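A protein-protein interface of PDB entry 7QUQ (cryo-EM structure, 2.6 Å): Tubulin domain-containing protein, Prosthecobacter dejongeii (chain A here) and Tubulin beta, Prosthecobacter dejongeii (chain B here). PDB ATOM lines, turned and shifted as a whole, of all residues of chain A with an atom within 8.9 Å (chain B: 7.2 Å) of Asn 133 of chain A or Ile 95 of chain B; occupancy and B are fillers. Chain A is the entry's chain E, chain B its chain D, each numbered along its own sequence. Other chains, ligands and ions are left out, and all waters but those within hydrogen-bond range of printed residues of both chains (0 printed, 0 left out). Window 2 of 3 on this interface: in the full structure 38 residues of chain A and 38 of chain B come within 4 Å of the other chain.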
ATOM      1  N   LYS A   2       6.351  -0.667 -16.430  1.00  0.00           N
ATOM      2  CA  LYS A   2       7.275  -1.694 -16.896  1.00  0.00           C
ATOM      3  C   LYS A   2       6.530  -2.839 -17.577  1.00  0.00           C
ATOM      4  O   LYS A   2       5.415  -3.187 -17.189  1.00  0.00           O
ATOM      5  CB  LYS A   2       8.117  -2.225 -15.733  1.00  0.00           C
ATOM      6  CG  LYS A   2       7.303  -2.738 -14.557  1.00  0.00           C
ATOM      7  CD  LYS A   2       8.175  -3.503 -13.575  1.00  0.00           C
ATOM      8  CE  LYS A   2       9.235  -2.603 -12.961  1.00  0.00           C
ATOM      9  NZ  LYS A   2       9.951  -3.273 -11.842  1.00  0.00           N
ATOM     10  N   VAL A   3       7.157  -3.417 -18.601  1.00  0.00           N
ATOM     11  CA  VAL A   3       6.560  -4.484 -19.387  1.00  0.00           C
ATOM     12  C   VAL A   3       7.420  -5.731 -19.250  1.00  0.00           C
ATOM     13  O   VAL A   3       8.533  -5.694 -18.719  1.00  0.00           O
ATOM     14  CB  VAL A   3       6.407  -4.094 -20.871  1.00  0.00           C
ATOM     15  CG1 VAL A   3       5.502  -2.878 -21.009  1.00  0.00           C
ATOM     16  CG2 VAL A   3       7.771  -3.831 -21.487  1.00  0.00           C
ATOM     17  N   ASN A   4       6.883  -6.852 -19.730  1.00  0.00           N
ATOM     18  CA  ASN A   4       7.621  -8.104 -19.686  1.00  0.00           C
ATOM     19  C   ASN A   4       8.845  -8.025 -20.590  1.00  0.00           C
ATOM     20  O   ASN A   4       8.806  -7.462 -21.686  1.00  0.00           O
ATOM     21  CB  ASN A   4       6.722  -9.272 -20.096  1.00  0.00           C
ATOM     22  CG  ASN A   4       6.313  -9.210 -21.552  1.00  0.00           C
ATOM     23  OD1 ASN A   4       6.952  -9.811 -22.415  1.00  0.00           O
ATOM     24  ND2 ASN A   4       5.237  -8.484 -21.834  1.00  0.00           N
ATOM     25  N   ASN A   5       9.946  -8.592 -20.111  1.00  0.00           N
ATOM     26  CA  ASN A   5      11.247  -8.389 -20.726  1.00  0.00           C
ATOM     27  C   ASN A   5      11.636  -9.584 -21.589  1.00  0.00           C
ATOM     28  O   ASN A   5      11.053 -10.668 -21.506  1.00  0.00           O
ATOM     29  CB  ASN A   5      12.303  -8.138 -19.648  1.00  0.00           C
ATOM     30  CG  ASN A   5      11.952  -6.963 -18.761  1.00  0.00           C
ATOM     31  OD1 ASN A   5      11.700  -7.128 -17.569  1.00  0.00           O
ATOM     32  ND2 ASN A   5      11.916  -5.770 -19.343  1.00  0.00           N
ATOM     33  N   THR A   6      12.637  -9.364 -22.438  1.00  0.00           N
ATOM     34  CA  THR A   6      13.169 -10.410 -23.301  1.00  0.00           C
ATOM     35  C   THR A   6      14.621 -10.096 -23.619  1.00  0.00           C
ATOM     36  O   THR A   6      14.938  -8.985 -24.055  1.00  0.00           O
ATOM     37  CB  THR A   6      12.360 -10.538 -24.598  1.00  0.00           C
ATOM     38  OG1 THR A   6      10.998 -10.861 -24.290  1.00  0.00           O
ATOM     39  CG2 THR A   6      12.941 -11.626 -25.486  1.00  0.00           C
ATOM     40  N   ILE A   7      15.496 -11.071 -23.393  1.00  0.00           N
ATOM     41  CA  ILE A   7      16.900 -10.998 -23.781  1.00  0.00           C
ATOM     42  C   ILE A   7      17.091 -11.825 -25.044  1.00  0.00           C
ATOM     43  O   ILE A   7      16.540 -12.926 -25.164  1.00  0.00           O
ATOM     44  CB  ILE A   7      17.833 -11.468 -22.648  1.00  0.00           C
ATOM     45  CG1 ILE A   7      19.291 -11.156 -22.986  1.00  0.00           C
ATOM     46  CG2 ILE A   7      17.637 -12.930 -22.303  1.00  0.00           C
ATOM     47  CD1 ILE A   7      20.215 -11.293 -21.822  1.00  0.00           C
ATOM     48  N   SER A  50      11.473  -1.278 -22.839  1.00  0.00           N
ATOM     49  CA  SER A  50      12.054  -2.089 -21.773  1.00  0.00           C
ATOM     50  C   SER A  50      11.898  -3.587 -22.001  1.00  0.00           C
ATOM     51  O   SER A  50      12.528  -4.369 -21.282  1.00  0.00           O
ATOM     52  CB  SER A  50      11.429  -1.708 -20.430  1.00  0.00           C
ATOM     53  OG  SER A  50      11.952  -2.502 -19.382  1.00  0.00           O
ATOM     54  N   SER A  51      11.075  -4.005 -22.965  1.00  0.00           N
ATOM     55  CA  SER A  51      10.951  -5.429 -23.259  1.00  0.00           C
ATOM     56  C   SER A  51      12.248  -5.992 -23.830  1.00  0.00           C
ATOM     57  O   SER A  51      12.656  -7.106 -23.479  1.00  0.00           O
ATOM     58  CB  SER A  51       9.795  -5.665 -24.227  1.00  0.00           C
ATOM     59  OG  SER A  51       9.986  -4.950 -25.434  1.00  0.00           O
ATOM     60  N   ARG A  67      19.293  -5.478 -25.004  1.00  0.00           N
ATOM     61  CA  ARG A  67      19.591  -6.589 -24.103  1.00  0.00           C
ATOM     62  C   ARG A  67      19.960  -7.809 -24.945  1.00  0.00           C
ATOM     63  O   ARG A  67      19.201  -8.767 -25.100  1.00  0.00           O
ATOM     64  CB  ARG A  67      18.419  -6.865 -23.170  1.00  0.00           C
ATOM     65  CG  ARG A  67      18.168  -5.752 -22.171  1.00  0.00           C
ATOM     66  CD  ARG A  67      16.997  -6.068 -21.263  1.00  0.00           C
ATOM     67  NE  ARG A  67      16.747  -4.987 -20.318  1.00  0.00           N
ATOM     68  CZ  ARG A  67      15.751  -4.974 -19.444  1.00  0.00           C
ATOM     69  NH1 ARG A  67      14.903  -5.982 -19.348  1.00  0.00           N
ATOM     70  NH2 ARG A  67      15.610  -3.924 -18.639  1.00  0.00           N
ATOM     71  N   GLU A 127      22.373  -9.559 -16.835  1.00  0.00           N
ATOM     72  CA  GLU A 127      21.248  -8.997 -17.575  1.00  0.00           C
ATOM     73  C   GLU A 127      19.909  -9.380 -16.950  1.00  0.00           C
ATOM     74  O   GLU A 127      19.025  -8.529 -16.805  1.00  0.00           O
ATOM     75  CB  GLU A 127      21.306  -9.448 -19.032  1.00  0.00           C
ATOM     76  CG  GLU A 127      22.166  -8.574 -19.925  1.00  0.00           C
ATOM     77  CD  GLU A 127      21.541  -7.218 -20.183  1.00  0.00           C
ATOM     78  OE1 GLU A 127      20.302  -7.105 -20.079  1.00  0.00           O
ATOM     79  OE2 GLU A 127      22.287  -6.265 -20.494  1.00  0.00           O
ATOM     80  N   ILE A 128      19.745 -10.648 -16.562  1.00  0.00           N
ATOM     81  CA  ILE A 128      18.468 -11.109 -16.018  1.00  0.00           C
ATOM     82  C   ILE A 128      18.196 -10.475 -14.660  1.00  0.00           C
ATOM     83  O   ILE A 128      17.058 -10.099 -14.354  1.00  0.00           O
ATOM     84  CB  ILE A 128      18.432 -12.647 -15.949  1.00  0.00           C
ATOM     85  CG1 ILE A 128      18.627 -13.248 -17.342  1.00  0.00           C
ATOM     86  CG2 ILE A 128      17.131 -13.136 -15.333  1.00  0.00           C
ATOM     87  CD1 ILE A 128      17.557 -12.854 -18.331  1.00  0.00           C
ATOM     88  N   ASP A 129      19.231 -10.336 -13.825  1.00  0.00           N
ATOM     89  CA  ASP A 129      19.067  -9.670 -12.540  1.00  0.00           C
ATOM     90  C   ASP A 129      18.670  -8.208 -12.691  1.00  0.00           C
ATOM     91  O   ASP A 129      18.126  -7.626 -11.747  1.00  0.00           O
ATOM     92  CB  ASP A 129      20.358  -9.775 -11.725  1.00  0.00           C
ATOM     93  CG  ASP A 129      20.593 -11.170 -11.186  1.00  0.00           C
ATOM     94  OD1 ASP A 129      19.604 -11.903 -10.982  1.00  0.00           O
ATOM     95  OD2 ASP A 129      21.769 -11.536 -10.974  1.00  0.00           O
ATOM     96  N   LYS A 130      18.928  -7.604 -13.850  1.00  0.00           N
ATOM     97  CA  LYS A 130      18.552  -6.224 -14.115  1.00  0.00           C
ATOM     98  C   LYS A 130      17.233  -6.135 -14.885  1.00  0.00           C
ATOM     99  O   LYS A 130      16.718  -5.034 -15.110  1.00  0.00           O
ATOM    100  CB  LYS A 130      19.699  -5.527 -14.865  1.00  0.00           C
ATOM    101  CG  LYS A 130      19.533  -4.038 -15.146  1.00  0.00           C
ATOM    102  CD  LYS A 130      20.752  -3.464 -15.841  1.00  0.00           C
ATOM    103  CE  LYS A 130      20.612  -1.963 -16.029  1.00  0.00           C
ATOM    104  NZ  LYS A 130      19.531  -1.627 -16.993  1.00  0.00           N
ATOM    105  N   CYS A 131      16.639  -7.273 -15.235  1.00  0.00           N
ATOM    106  CA  CYS A 131      15.335  -7.285 -15.883  1.00  0.00           C
ATOM    107  C   CYS A 131      14.230  -7.113 -14.851  1.00  0.00           C
ATOM    108  O   CYS A 131      14.344  -7.557 -13.705  1.00  0.00           O
ATOM    109  CB  CYS A 131      15.106  -8.584 -16.659  1.00  0.00           C
ATOM    110  SG  CYS A 131      16.191  -8.846 -18.075  1.00  0.00           S
ATOM    111  N   ASP A 132      13.148  -6.462 -15.274  1.00  0.00           N
ATOM    112  CA  ASP A 132      11.996  -6.285 -14.398  1.00  0.00           C
ATOM    113  C   ASP A 132      11.243  -7.599 -14.238  1.00  0.00           C
ATOM    114  O   ASP A 132      11.148  -8.146 -13.133  1.00  0.00           O
ATOM    115  CB  ASP A 132      11.078  -5.197 -14.959  1.00  0.00           C
ATOM    116  CG  ASP A 132      11.778  -3.858 -15.095  1.00  0.00           C
ATOM    117  OD1 ASP A 132      12.727  -3.600 -14.325  1.00  0.00           O
ATOM    118  OD2 ASP A 132      11.380  -3.067 -15.975  1.00  0.00           O
ATOM    119  N   ASN A 133      10.704  -8.124 -15.339  1.00  0.00           N
ATOM    120  CA  ASN A 133      10.138  -9.474 -15.381  1.00  0.00           C
ATOM    121  C   ASN A 133      10.485 -10.046 -16.752  1.00  0.00           C
ATOM    122  O   ASN A 133       9.756  -9.834 -17.725  1.00  0.00           O
ATOM    123  CB  ASN A 133       8.636  -9.476 -15.140  1.00  0.00           C
ATOM    124  CG  ASN A 133       8.072 -10.880 -14.986  1.00  0.00           C
ATOM    125  OD1 ASN A 133       8.805 -11.867 -15.037  1.00  0.00           O
ATOM    126  ND2 ASN A 133       6.761 -10.974 -14.809  1.00  0.00           N
ATOM    127  N   VAL A 134      11.593 -10.769 -16.822  1.00  0.00           N
ATOM    128  CA  VAL A 134      11.958 -11.451 -18.056  1.00  0.00           C
ATOM    129  C   VAL A 134      11.010 -12.626 -18.272  1.00  0.00           C
ATOM    130  O   VAL A 134      10.878 -13.514 -17.419  1.00  0.00           O
ATOM    131  CB  VAL A 134      13.443 -11.866 -18.039  1.00  0.00           C
ATOM    132  CG1 VAL A 134      13.760 -12.854 -16.922  1.00  0.00           C
ATOM    133  CG2 VAL A 134      13.846 -12.439 -19.390  1.00  0.00           C
ATOM    134  N   GLY A 135      10.288 -12.595 -19.386  1.00  0.00           N
ATOM    135  CA  GLY A 135       9.303 -13.614 -19.677  1.00  0.00           C
ATOM    136  C   GLY A 135       9.643 -14.379 -20.933  1.00  0.00           C
ATOM    137  O   GLY A 135       8.772 -14.998 -21.551  1.00  0.00           O
ATOM    138  N   GLY A 136      10.912 -14.338 -21.323  1.00  0.00           N
ATOM    139  CA  GLY A 136      11.346 -15.028 -22.517  1.00  0.00           C
ATOM    140  C   GLY A 136      12.774 -14.732 -22.916  1.00  0.00           C
ATOM    141  O   GLY A 136      13.270 -13.622 -22.709  1.00  0.00           O
ATOM    142  N   GLU A 165      11.849 -21.068 -14.724  1.00  0.00           N
ATOM    143  CA  GLU A 165      10.686 -20.196 -14.771  1.00  0.00           C
ATOM    144  C   GLU A 165      10.688 -19.290 -15.993  1.00  0.00           C
ATOM    145  O   GLU A 165       9.698 -18.587 -16.228  1.00  0.00           O
ATOM    146  CB  GLU A 165      10.615 -19.350 -13.495  1.00  0.00           C
ATOM    147  CG  GLU A 165      11.364 -18.024 -13.574  1.00  0.00           C
ATOM    148  CD  GLU A 165      12.842 -18.156 -13.254  1.00  0.00           C
ATOM    149  OE1 GLU A 165      13.303 -19.290 -13.006  1.00  0.00           O
ATOM    150  OE2 GLU A 165      13.543 -17.123 -13.254  1.00  0.00           O
ATOM    151  N   ILE A 166      11.759 -19.302 -16.777  1.00  0.00           N
ATOM    152  CA  ILE A 166      11.952 -18.371 -17.884  1.00  0.00           C
ATOM    153  C   ILE A 166      11.659 -19.107 -19.188  1.00  0.00           C
ATOM    154  O   ILE A 166      12.327 -20.110 -19.478  1.00  0.00           O
ATOM    155  CB  ILE A 166      13.374 -17.798 -17.894  1.00  0.00           C
ATOM    156  CG1 ILE A 166      13.589 -16.863 -16.704  1.00  0.00           C
ATOM    157  CG2 ILE A 166      13.626 -17.056 -19.188  1.00  0.00           C
ATOM    158  CD1 ILE A 166      14.958 -16.224 -16.687  1.00  0.00           C
ATOM    159  N   PRO A 167      10.685 -18.666 -19.979  1.00  0.00           N
ATOM    160  CA  PRO A 167      10.475 -19.267 -21.300  1.00  0.00           C
ATOM    161  C   PRO A 167      11.655 -19.018 -22.225  1.00  0.00           C
ATOM    162  O   PRO A 167      12.369 -18.021 -22.104  1.00  0.00           O
ATOM    163  CB  PRO A 167       9.214 -18.563 -21.813  1.00  0.00           C
ATOM    164  CG  PRO A 167       8.535 -18.047 -20.588  1.00  0.00           C
ATOM    165  CD  PRO A 167       9.637 -17.690 -19.642  1.00  0.00           C
ATOM    166  N   SER A 255       2.878 -11.203 -24.442  1.00  0.00           N
ATOM    167  CA  SER A 255       4.173 -11.558 -23.889  1.00  0.00           C
ATOM    168  C   SER A 255       4.748 -12.749 -24.649  1.00  0.00           C
ATOM    169  O   SER A 255       4.048 -13.445 -25.390  1.00  0.00           O
ATOM    170  CB  SER A 255       4.051 -11.884 -22.402  1.00  0.00           C
ATOM    171  OG  SER A 255       5.320 -12.146 -21.831  1.00  0.00           O
ATOM    172  N   LEU A 256       6.051 -12.978 -24.473  1.00  0.00           N
ATOM    173  CA  LEU A 256       6.637 -14.174 -25.065  1.00  0.00           C
ATOM    174  C   LEU A 256       6.080 -15.425 -24.400  1.00  0.00           C
ATOM    175  O   LEU A 256       5.974 -16.469 -25.047  1.00  0.00           O
ATOM    176  CB  LEU A 256       8.166 -14.124 -24.980  1.00  0.00           C
ATOM    177  CG  LEU A 256       9.003 -15.192 -25.706  1.00  0.00           C
ATOM    178  CD1 LEU A 256      10.368 -14.614 -26.046  1.00  0.00           C
ATOM    179  CD2 LEU A 256       9.179 -16.498 -24.933  1.00  0.00           C
ATOM    180  N   ARG A 257       5.703 -15.337 -23.121  1.00  0.00           N
ATOM    181  CA  ARG A 257       4.986 -16.442 -22.492  1.00  0.00           C
ATOM    182  C   ARG A 257       3.540 -16.510 -22.973  1.00  0.00           C
ATOM    183  O   ARG A 257       2.976 -17.600 -23.088  1.00  0.00           O
ATOM    184  CB  ARG A 257       5.040 -16.323 -20.970  1.00  0.00           C
ATOM    185  CG  ARG A 257       4.704 -17.625 -20.259  1.00  0.00           C
ATOM    186  CD  ARG A 257       4.425 -17.414 -18.783  1.00  0.00           C
ATOM    187  NE  ARG A 257       5.607 -16.964 -18.060  1.00  0.00           N
ATOM    188  CZ  ARG A 257       6.572 -17.766 -17.632  1.00  0.00           C
ATOM    189  NH1 ARG A 257       6.530 -19.071 -17.846  1.00  0.00           N
ATOM    190  NH2 ARG A 257       7.603 -17.247 -16.971  1.00  0.00           N
ATOM    191  N   ASP B  68      -4.563  -5.469 -13.810  1.00  0.00           N
ATOM    192  CA  ASP B  68      -4.351  -6.280 -15.002  1.00  0.00           C
ATOM    193  C   ASP B  68      -2.918  -6.776 -14.976  1.00  0.00           C
ATOM    194  O   ASP B  68      -1.987  -5.966 -15.018  1.00  0.00           O
ATOM    195  CB  ASP B  68      -4.624  -5.467 -16.271  1.00  0.00           C
ATOM    196  CG  ASP B  68      -4.424  -6.274 -17.537  1.00  0.00           C
ATOM    197  OD1 ASP B  68      -4.619  -7.506 -17.495  1.00  0.00           O
ATOM    198  OD2 ASP B  68      -4.073  -5.677 -18.575  1.00  0.00           O
ATOM    199  N   LEU B  69      -2.740  -8.092 -14.880  1.00  0.00           N
ATOM    200  CA  LEU B  69      -1.424  -8.672 -15.096  1.00  0.00           C
ATOM    201  C   LEU B  69      -0.959  -8.332 -16.506  1.00  0.00           C
ATOM    202  O   LEU B  69      -1.743  -8.373 -17.459  1.00  0.00           O
ATOM    203  CB  LEU B  69      -1.461 -10.189 -14.900  1.00  0.00           C
ATOM    204  CG  LEU B  69      -1.583 -10.799 -13.500  1.00  0.00           C
ATOM    205  CD1 LEU B  69      -2.993 -10.688 -12.950  1.00  0.00           C
ATOM    206  CD2 LEU B  69      -1.146 -12.251 -13.535  1.00  0.00           C
ATOM    207  N   GLU B  70       0.333  -7.991 -16.632  1.00  0.00           N
ATOM    208  CA  GLU B  70       0.867  -7.371 -17.842  1.00  0.00           C
ATOM    209  C   GLU B  70       0.001  -6.158 -18.159  1.00  0.00           C
ATOM    210  O   GLU B  70      -0.857  -6.225 -19.047  1.00  0.00           O
ATOM    211  CB  GLU B  70       0.899  -8.362 -19.012  1.00  0.00           C
ATOM    212  CG  GLU B  70       1.548  -7.830 -20.283  1.00  0.00           C
ATOM    213  CD  GLU B  70       1.351  -8.761 -21.463  1.00  0.00           C
ATOM    214  OE1 GLU B  70       0.191  -9.139 -21.732  1.00  0.00           O
ATOM    215  OE2 GLU B  70       2.351  -9.108 -22.125  1.00  0.00           O
ATOM    216  N   PRO B  71       0.138  -5.057 -17.398  1.00  0.00           N
ATOM    217  CA  PRO B  71      -0.857  -3.976 -17.470  1.00  0.00           C
ATOM    218  C   PRO B  71      -1.004  -3.347 -18.848  1.00  0.00           C
ATOM    219  O   PRO B  71      -2.074  -3.447 -19.454  1.00  0.00           O
ATOM    220  CB  PRO B  71      -0.335  -2.954 -16.451  1.00  0.00           C
ATOM    221  CG  PRO B  71       1.124  -3.253 -16.310  1.00  0.00           C
ATOM    222  CD  PRO B  71       1.262  -4.730 -16.503  1.00  0.00           C
ATOM    223  N   VAL B  92      -3.396  -0.913  -9.771  1.00  0.00           N
ATOM    224  CA  VAL B  92      -2.011  -1.366  -9.752  1.00  0.00           C
ATOM    225  C   VAL B  92      -1.604  -1.795 -11.157  1.00  0.00           C
ATOM    226  O   VAL B  92      -2.396  -2.389 -11.896  1.00  0.00           O
ATOM    227  CB  VAL B  92      -1.801  -2.506  -8.726  1.00  0.00           C
ATOM    228  CG1 VAL B  92      -2.621  -3.735  -9.086  1.00  0.00           C
ATOM    229  CG2 VAL B  92      -0.322  -2.858  -8.598  1.00  0.00           C
ATOM    230  N   ARG B  93      -0.375  -1.452 -11.533  1.00  0.00           N
ATOM    231  CA  ARG B  93       0.266  -1.987 -12.731  1.00  0.00           C
ATOM    232  C   ARG B  93       1.167  -3.121 -12.255  1.00  0.00           C
ATOM    233  O   ARG B  93       2.343  -2.921 -11.949  1.00  0.00           O
ATOM    234  CB  ARG B  93       1.039  -0.903 -13.475  1.00  0.00           C
ATOM    235  CG  ARG B  93       0.153   0.078 -14.223  1.00  0.00           C
ATOM    236  CD  ARG B  93       0.971   1.001 -15.111  1.00  0.00           C
ATOM    237  NE  ARG B  93       0.344   2.309 -15.253  1.00  0.00           N
ATOM    238  CZ  ARG B  93       0.960   3.389 -15.715  1.00  0.00           C
ATOM    239  NH1 ARG B  93       2.225   3.351 -16.099  1.00  0.00           N
ATOM    240  NH2 ARG B  93       0.288   4.534 -15.797  1.00  0.00           N
ATOM    241  N   LYS B  94       0.594  -4.320 -12.181  1.00  0.00           N
ATOM    242  CA  LYS B  94       1.275  -5.475 -11.614  1.00  0.00           C
ATOM    243  C   LYS B  94       2.480  -5.861 -12.474  1.00  0.00           C
ATOM    244  O   LYS B  94       2.579  -5.515 -13.655  1.00  0.00           O
ATOM    245  CB  LYS B  94       0.293  -6.642 -11.473  1.00  0.00           C
ATOM    246  CG  LYS B  94       0.863  -7.882 -10.793  1.00  0.00           C
ATOM    247  CD  LYS B  94      -0.148  -8.992 -10.630  1.00  0.00           C
ATOM    248  CE  LYS B  94       0.544 -10.251 -10.129  1.00  0.00           C
ATOM    249  NZ  LYS B  94       1.115 -10.075  -8.766  1.00  0.00           N
ATOM    250  N   ILE B  95       3.423  -6.561 -11.848  1.00  0.00           N
ATOM    251  CA  ILE B  95       4.529  -7.191 -12.574  1.00  0.00           C
ATOM    252  C   ILE B  95       3.954  -8.098 -13.657  1.00  0.00           C
ATOM    253  O   ILE B  95       3.037  -8.894 -13.375  1.00  0.00           O
ATOM    254  CB  ILE B  95       5.424  -7.984 -11.604  1.00  0.00           C
ATOM    255  CG1 ILE B  95       6.077  -7.047 -10.583  1.00  0.00           C
ATOM    256  CG2 ILE B  95       6.484  -8.757 -12.354  1.00  0.00           C
ATOM    257  CD1 ILE B  95       5.393  -7.034  -9.229  1.00  0.00           C
ATOM    258  N   PRO B  96       4.424  -8.001 -14.900  1.00  0.00           N
ATOM    259  CA  PRO B  96       3.769  -8.707 -16.011  1.00  0.00           C
ATOM    260  C   PRO B  96       3.868 -10.219 -15.888  1.00  0.00           C
ATOM    261  O   PRO B  96       4.420 -10.777 -14.936  1.00  0.00           O
ATOM    262  CB  PRO B  96       4.522  -8.215 -17.255  1.00  0.00           C
ATOM    263  CG  PRO B  96       5.451  -7.146 -16.795  1.00  0.00           C
ATOM    264  CD  PRO B  96       5.245  -6.870 -15.355  1.00  0.00           C
ATOM    265  N   GLY B  97       3.319 -10.893 -16.893  1.00  0.00           N
ATOM    266  CA  GLY B  97       3.238 -12.338 -16.869  1.00  0.00           C
ATOM    267  C   GLY B  97       1.808 -12.835 -16.889  1.00  0.00           C
ATOM    268  O   GLY B  97       1.487 -13.841 -16.254  1.00  0.00           O
ATOM    269  N   ALA B  98       0.931 -12.113 -17.592  1.00  0.00           N
ATOM    270  CA  ALA B  98      -0.465 -12.528 -17.678  1.00  0.00           C
ATOM    271  C   ALA B  98      -0.626 -13.800 -18.501  1.00  0.00           C
ATOM    272  O   ALA B  98      -1.376 -14.703 -18.110  1.00  0.00           O
ATOM    273  CB  ALA B  98      -1.308 -11.408 -18.281  1.00  0.00           C
ATOM    274  N   GLU B 109       0.536 -16.172 -10.443  1.00  0.00           N
ATOM    275  CA  GLU B 109       0.653 -14.790 -10.007  1.00  0.00           C
ATOM    276  C   GLU B 109      -0.634 -14.258  -9.398  1.00  0.00           C
ATOM    277  O   GLU B 109      -0.660 -13.111  -8.940  1.00  0.00           O
ATOM    278  CB  GLU B 109       1.088 -13.885 -11.168  1.00  0.00           C
ATOM    279  CG  GLU B 109       2.578 -13.925 -11.470  1.00  0.00           C
ATOM    280  CD  GLU B 109       2.949 -15.040 -12.419  1.00  0.00           C
ATOM    281  OE1 GLU B 109       2.036 -15.752 -12.877  1.00  0.00           O
ATOM    282  OE2 GLU B 109       4.154 -15.205 -12.708  1.00  0.00           O
ATOM    283  N   LYS B 112      -0.009 -14.014  -5.476  1.00  0.00           N
ATOM    284  CA  LYS B 112       0.862 -12.935  -5.031  1.00  0.00           C
ATOM    285  C   LYS B 112       0.248 -11.558  -5.251  1.00  0.00           C
ATOM    286  O   LYS B 112       0.922 -10.549  -5.018  1.00  0.00           O
ATOM    287  CB  LYS B 112       2.221 -13.019  -5.731  1.00  0.00           C
ATOM    288  CG  LYS B 112       2.168 -12.878  -7.241  1.00  0.00           C
ATOM    289  CD  LYS B 112       3.566 -12.856  -7.839  1.00  0.00           C
ATOM    290  CE  LYS B 112       4.270 -14.192  -7.668  1.00  0.00           C
ATOM    291  NZ  LYS B 112       3.612 -15.276  -8.443  1.00  0.00           N
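Printed residues of chain A that touch a printed residue of chain B: Lys 2, Val 3, Asn 4, Asn 133 and Ser 255.
Printed residues of chain B that touch a printed residue of chain A: Glu 70, Ile 95 and Pro 96.
Along chain B the printed residues that touch a printed residue of chain A span positions 70 to 96.
Among the printed residues, 7 pairs touch across the chains.
The side-chain hydroxyl (OG) of Ser 255 of chain A is in hydrogen-bond range of the side-chain amide oxygen (OD1) of Asn 4 of chain A (2.9 Å).
OD1 of Asn 5 of chain A lies within hydrogen-bond range of N of Asn 133 of chain A, 2.6 Å away.
The backbone NH (N) of Arg 257 of chain A sits close to the side-chain hydroxyl (OG) of Ser 255 of chain A, 3.5 Å away.
The side-chain amino group (NZ) of Lys 2 of chain A is in salt-bridge range of the side-chain carboxylate (OD1) of Asp 132 of chain A (3.7 Å).
The side-chain amide nitrogen of Asn 5 of chain A sits at hydrogen-bond distance from the backbone carbonyl oxygen of Val 3 of chain A, 3.4 Å away.
Lys 2 of chain A touches Pro 96 of chain B (O to CG, 3.98 Å).
Val 3 of chain A touches Pro 96 of chain B (C to CG, 3.5 Å).
N of Asn 4 of chain A touches CG of Pro 96 of chain B, 3.3 Å away.
ND2 of Asn 133 of chain A touches CG2 of Ile 95 of chain B (3.3 Å).
N of Ser 255 of chain A sits at hydrogen-bond distance from OE2 of Glu 70 of chain B (3.2 Å).
The side-chain carboxylate of Glu 70 of chain B is in hydrogen-bond range of the side-chain amide nitrogen of Asn 4 of chain A (3.0 Å).
The backbone carbonyl oxygen (O) of Pro 96 of chain B lies close to the side-chain amide nitrogen (ND2) of Asn 133 of chain A (2.4 Å).
Of chain B, only Ile 95 (3.3 Å) and Pro 96 (2.4 Å) come within 4 Å of Asn 133 of chain A.
Ile 95 of chain B touches just one residue of chain A: Asn 133.
Pro 96 of chain B touches just these residues of chain A: Lys 2, Val 3, Asn 4 and Asn 133.
Printed residues of chain A within 4 Å of Glu 70 of chain B: Asn 4 (3.0 Å) and Ser 255 (3.2 Å).
Printed residues of chain B within 4 Å of Asn 4 of chain A: Glu 70 (3.0 Å) and Pro 96 (3.3 Å).
Printed residues of chain B within 4 Å of Val 3 of chain A: Pro 96 (3.5 Å).
Pro 167 of chain A touches none of the printed residues of chain B.
Pro 71 of chain B touches none of the printed residues of chain A.
The nearest residue of chain B that does not touch Asn 133 of chain A is Gly 97 of chain B (4.02 Å).
The nearest printed residue of chain B that does not touch Ser 255 of chain A is Gly 97 of chain B (5.4 Å).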
